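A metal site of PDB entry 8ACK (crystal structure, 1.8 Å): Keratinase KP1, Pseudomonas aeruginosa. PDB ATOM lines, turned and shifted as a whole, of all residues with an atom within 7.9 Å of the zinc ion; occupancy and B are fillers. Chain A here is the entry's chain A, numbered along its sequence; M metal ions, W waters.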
ATOM      1  N   ILE A 354      13.351   7.359  33.348  1.00  0.00           N
ATOM      2  CA  ILE A 354      12.331   7.538  32.322  1.00  0.00           C
ATOM      3  C   ILE A 354      13.039   7.785  30.985  1.00  0.00           C
ATOM      4  O   ILE A 354      13.973   8.585  30.924  1.00  0.00           O
ATOM      5  CB  ILE A 354      11.391   8.701  32.660  1.00  0.00           C
ATOM      6  CG1 ILE A 354      10.686   8.445  33.994  1.00  0.00           C
ATOM      7  CG2 ILE A 354      10.377   8.915  31.537  1.00  0.00           C
ATOM      8  CD1 ILE A 354       9.992   9.703  34.586  1.00  0.00           C
ATOM      9  N   TYR A 355      12.592   7.100  29.930  1.00  0.00           N
ATOM     10  CA  TYR A 355      13.191   7.301  28.617  1.00  0.00           C
ATOM     11  C   TYR A 355      13.193   8.783  28.273  1.00  0.00           C
ATOM     12  O   TYR A 355      12.173   9.464  28.382  1.00  0.00           O
ATOM     13  CB  TYR A 355      12.429   6.527  27.539  1.00  0.00           C
ATOM     14  CG  TYR A 355      12.615   5.035  27.559  1.00  0.00           C
ATOM     15  CD1 TYR A 355      13.274   4.403  28.601  1.00  0.00           C
ATOM     16  CD2 TYR A 355      12.108   4.239  26.540  1.00  0.00           C
ATOM     17  CE1 TYR A 355      13.438   3.024  28.626  1.00  0.00           C
ATOM     18  CE2 TYR A 355      12.255   2.870  26.550  1.00  0.00           C
ATOM     19  CZ  TYR A 355      12.924   2.266  27.587  1.00  0.00           C
ATOM     20  OH  TYR A 355      13.078   0.904  27.587  1.00  0.00           O
ATOM     21  N   ASP A 356      14.360   9.278  27.849  1.00  0.00           N
ATOM     22  CA  ASP A 356      14.544  10.712  27.597  1.00  0.00           C
ATOM     23  C   ASP A 356      14.050  11.073  26.186  1.00  0.00           C
ATOM     24  O   ASP A 356      14.811  11.479  25.305  1.00  0.00           O
ATOM     25  CB  ASP A 356      16.000  11.097  27.798  1.00  0.00           C
ATOM     26  CG  ASP A 356      16.257  12.567  27.548  1.00  0.00           C
ATOM     27  OD1 ASP A 356      15.383  13.396  27.886  1.00  0.00           O
ATOM     28  OD2 ASP A 356      17.330  12.903  27.009  1.00  0.00           O
ATOM     29  N   GLY A 357      12.740  10.925  25.993  1.00  0.00           N
ATOM     30  CA  GLY A 357      12.166  11.136  24.678  1.00  0.00           C
ATOM     31  C   GLY A 357      12.401  12.523  24.103  1.00  0.00           C
ATOM     32  O   GLY A 357      12.554  12.681  22.886  1.00  0.00           O
ATOM     33  N   ASP A 358      12.429  13.547  24.957  1.00  0.00           N
ATOM     34  CA  ASP A 358      12.619  14.923  24.497  1.00  0.00           C
ATOM     35  C   ASP A 358      14.084  15.286  24.296  1.00  0.00           C
ATOM     36  O   ASP A 358      14.378  16.423  23.916  1.00  0.00           O
ATOM     37  CB  ASP A 358      11.965  15.910  25.484  1.00  0.00           C
ATOM     38  CG  ASP A 358      12.665  15.942  26.834  1.00  0.00           C
ATOM     39  OD1 ASP A 358      13.570  15.121  27.075  1.00  0.00           O
ATOM     40  OD2 ASP A 358      12.294  16.790  27.673  1.00  0.00           O
ATOM     41  N   GLY A 359      15.011  14.357  24.545  1.00  0.00           N
ATOM     42  CA  GLY A 359      16.422  14.641  24.357  1.00  0.00           C
ATOM     43  C   GLY A 359      17.018  15.659  25.308  1.00  0.00           C
ATOM     44  O   GLY A 359      18.124  16.143  25.045  1.00  0.00           O
ATOM     45  N   SER A 360      16.328  15.997  26.394  1.00  0.00           N
ATOM     46  CA  SER A 360      16.790  17.058  27.282  1.00  0.00           C
ATOM     47  C   SER A 360      18.066  16.685  28.034  1.00  0.00           C
ATOM     48  O   SER A 360      18.808  17.585  28.449  1.00  0.00           O
ATOM     49  CB  SER A 360      15.676  17.427  28.277  1.00  0.00           C
ATOM     50  OG  SER A 360      15.466  16.378  29.214  1.00  0.00           O
ATOM     51  N   ASP A 361      18.344  15.401  28.216  1.00  0.00           N
ATOM     52  CA  ASP A 361      19.533  14.958  28.926  1.00  0.00           C
ATOM     53  C   ASP A 361      20.659  14.525  27.997  1.00  0.00           C
ATOM     54  O   ASP A 361      21.822  14.873  28.237  1.00  0.00           O
ATOM     55  CB  ASP A 361      19.182  13.796  29.856  1.00  0.00           C
ATOM     56  CG  ASP A 361      18.299  14.235  31.006  1.00  0.00           C
ATOM     57  OD1 ASP A 361      18.492  15.358  31.518  1.00  0.00           O
ATOM     58  OD2 ASP A 361      17.399  13.457  31.384  1.00  0.00           O
ATOM     59  N   PHE A 362      20.355  13.777  26.943  1.00  0.00           N
ATOM     60  CA  PHE A 362      21.379  13.148  26.123  1.00  0.00           C
ATOM     61  C   PHE A 362      21.351  13.569  24.648  1.00  0.00           C
ATOM     62  O   PHE A 362      22.168  13.066  23.869  1.00  0.00           O
ATOM     63  CB  PHE A 362      21.255  11.625  26.241  1.00  0.00           C
ATOM     64  CG  PHE A 362      21.201  11.148  27.667  1.00  0.00           C
ATOM     65  CD1 PHE A 362      22.348  11.106  28.433  1.00  0.00           C
ATOM     66  CD2 PHE A 362      20.004  10.781  28.238  1.00  0.00           C
ATOM     67  CE1 PHE A 362      22.300  10.689  29.756  1.00  0.00           C
ATOM     68  CE2 PHE A 362      19.944  10.363  29.554  1.00  0.00           C
ATOM     69  CZ  PHE A 362      21.098  10.302  30.313  1.00  0.00           C
ATOM     70  N   LEU A 364      19.372  13.075  22.098  1.00  0.00           N
ATOM     71  CA  LEU A 364      18.668  12.266  21.113  1.00  0.00           C
ATOM     72  C   LEU A 364      17.170  12.345  21.388  1.00  0.00           C
ATOM     73  O   LEU A 364      16.705  11.939  22.464  1.00  0.00           O
ATOM     74  CB  LEU A 364      19.133  10.811  21.140  1.00  0.00           C
ATOM     75  CG  LEU A 364      18.521   9.862  20.106  1.00  0.00           C
ATOM     76  CD1 LEU A 364      18.727  10.368  18.683  1.00  0.00           C
ATOM     77  CD2 LEU A 364      19.081   8.454  20.250  1.00  0.00           C
ATOM     78  N   SER A 370       7.077  11.482  21.486  1.00  0.00           N
ATOM     79  CA  SER A 370       7.871  10.869  22.544  1.00  0.00           C
ATOM     80  C   SER A 370       8.038  11.840  23.712  1.00  0.00           C
ATOM     81  O   SER A 370       8.026  11.414  24.876  1.00  0.00           O
ATOM     82  CB  SER A 370       9.238  10.450  21.996  1.00  0.00           C
ATOM     83  OG  SER A 370       9.110   9.569  20.895  1.00  0.00           O
ATOM     84  N   ALA A 371       8.188  13.129  23.429  1.00  0.00           N
ATOM     85  CA  ALA A 371       8.303  14.091  24.512  1.00  0.00           C
ATOM     86  C   ALA A 371       7.068  14.067  25.398  1.00  0.00           C
ATOM     87  O   ALA A 371       7.181  14.094  26.632  1.00  0.00           O
ATOM     88  CB  ALA A 371       8.522  15.499  23.957  1.00  0.00           C
ATOM     89  N   GLU A 374       7.045  10.911  27.624  1.00  0.00           N
ATOM     90  CA  GLU A 374       7.989  11.141  28.714  1.00  0.00           C
ATOM     91  C   GLU A 374       7.399  12.071  29.766  1.00  0.00           C
ATOM     92  O   GLU A 374       7.606  11.874  30.971  1.00  0.00           O
ATOM     93  CB  GLU A 374       9.279  11.711  28.133  1.00  0.00           C
ATOM     94  CG  GLU A 374      10.317  12.145  29.148  1.00  0.00           C
ATOM     95  CD  GLU A 374      11.445  12.944  28.519  1.00  0.00           C
ATOM     96  OE1 GLU A 374      11.233  13.567  27.462  1.00  0.00           O
ATOM     97  OE2 GLU A 374      12.548  12.983  29.104  1.00  0.00           O
ATOM     98  N   ARG A 375       6.685  13.108  29.324  1.00  0.00           N
ATOM     99  CA  ARG A 375       6.077  14.066  30.250  1.00  0.00           C
ATOM    100  C   ARG A 375       4.986  13.413  31.102  1.00  0.00           C
ATOM    101  O   ARG A 375       4.840  13.749  32.280  1.00  0.00           O
ATOM    102  CB  ARG A 375       5.520  15.246  29.459  1.00  0.00           C
ATOM    103  CG  ARG A 375       5.517  16.557  30.196  1.00  0.00           C
ATOM    104  CD  ARG A 375       5.241  17.705  29.233  1.00  0.00           C
ATOM    105  NE  ARG A 375       6.408  18.037  28.415  1.00  0.00           N
ATOM    106  CZ  ARG A 375       6.491  17.816  27.102  1.00  0.00           C
ATOM    107  NH1 ARG A 375       5.481  17.267  26.441  1.00  0.00           N
ATOM    108  NH2 ARG A 375       7.594  18.147  26.447  1.00  0.00           N
ATOM    109  N   GLU A 378       6.832  11.543  33.747  1.00  0.00           N
ATOM    110  CA  GLU A 378       7.433  12.488  34.687  1.00  0.00           C
ATOM    111  C   GLU A 378       6.388  13.027  35.648  1.00  0.00           C
ATOM    112  O   GLU A 378       6.632  13.122  36.848  1.00  0.00           O
ATOM    113  CB  GLU A 378       8.111  13.652  33.945  1.00  0.00           C
ATOM    114  CG  GLU A 378       9.388  13.260  33.203  1.00  0.00           C
ATOM    115  CD  GLU A 378       9.891  14.369  32.287  1.00  0.00           C
ATOM    116  OE1 GLU A 378      11.062  14.299  31.859  1.00  0.00           O
ATOM    117  OE2 GLU A 378       9.118  15.301  31.990  1.00  0.00           O
ATOM    118  N   GLU A 389      14.575  10.609  36.770  1.00  0.00           N
ATOM    119  CA  GLU A 389      15.518  11.262  35.869  1.00  0.00           C
ATOM    120  C   GLU A 389      15.558  10.514  34.552  1.00  0.00           C
ATOM    121  O   GLU A 389      14.960   9.446  34.407  1.00  0.00           O
ATOM    122  CB  GLU A 389      16.918  11.356  36.494  1.00  0.00           C
ATOM    123  CG  GLU A 389      17.629   9.993  36.688  1.00  0.00           C
ATOM    124  CD  GLU A 389      18.839  10.151  37.610  1.00  0.00           C
ATOM    125  OE1 GLU A 389      18.640  10.202  38.852  1.00  0.00           O
ATOM    126  OE2 GLU A 389      19.977  10.251  37.108  1.00  0.00           O
ATOM    127  N   GLY A 390      16.246  11.098  33.566  1.00  0.00           N
ATOM    128  CA  GLY A 390      16.233  10.537  32.237  1.00  0.00           C
ATOM    129  C   GLY A 390      17.256   9.430  32.043  1.00  0.00           C
ATOM    130  O   GLY A 390      18.262   9.346  32.757  1.00  0.00           O
ATOM    131  N   THR A 391      16.994   8.573  31.056  1.00  0.00           N
ATOM    132  CA  THR A 391      17.960   7.581  30.609  1.00  0.00           C
ATOM    133  C   THR A 391      17.978   7.565  29.090  1.00  0.00           C
ATOM    134  O   THR A 391      17.036   8.007  28.436  1.00  0.00           O
ATOM    135  CB  THR A 391      17.654   6.176  31.164  1.00  0.00           C
ATOM    136  OG1 THR A 391      18.733   5.275  30.853  1.00  0.00           O
ATOM    137  CG2 THR A 391      16.360   5.628  30.572  1.00  0.00           C
HETATM  138 ZN    ZN M   1      13.989  14.416  28.943  1.00  0.00          ZN
HETATM  139  O   HOH W   1      14.907  14.074  30.587  1.00  0.00           O
HETATM  140  O   HOH W   2      12.678  15.737  30.274  1.00  0.00           O
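The side-chain carboxylate of Asp 356 is in hydrogen-bond range of the backbone NH of Asp 361, 3.0 Å away.
The side-chain carboxylate (OD1) of Asp 356 sits close to the backbone NH (N) of Gly 359 (3.5 Å).
The side-chain carboxylate (OD2) of Asp 356 sits at hydrogen-bond distance from the backbone NH (N) of Phe 362, at 3.1 Å.
The backbone NH of Asp 356 lies within hydrogen-bond range of the backbone carbonyl oxygen of Thr 391 (3.0 Å).
OE1 of Glu 374 is in hydrogen-bond range of N of Gly 357, 3.4 Å away.
Four residues have an atom within 4 Å of the zinc ion: Asp 356, Asp 358, Ser 360 and Glu 374.
The nearest printed residue that does not touch the zinc ion is Glu 378 (4.1 Å).
Water W2 bridges the side-chain carboxylate of Glu 378 (2.7 Å) and the side-chain carboxylate of Asp 358 (2.8 Å).
The zinc ion is bound by water W1 (1.9 Å), the side-chain carboxylate (OD1) of Asp 356 (2.0 Å), the side-chain carboxylate (OE2) of Glu 374 (2.0 Å), the side-chain carboxylate (OD1) of Asp 358 (2.0 Å), water W2 (2.3 Å) and the side-chain hydroxyl (OG) of Ser 360 (2.5 Å).
The zinc ion has six donor atoms within binding distance.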
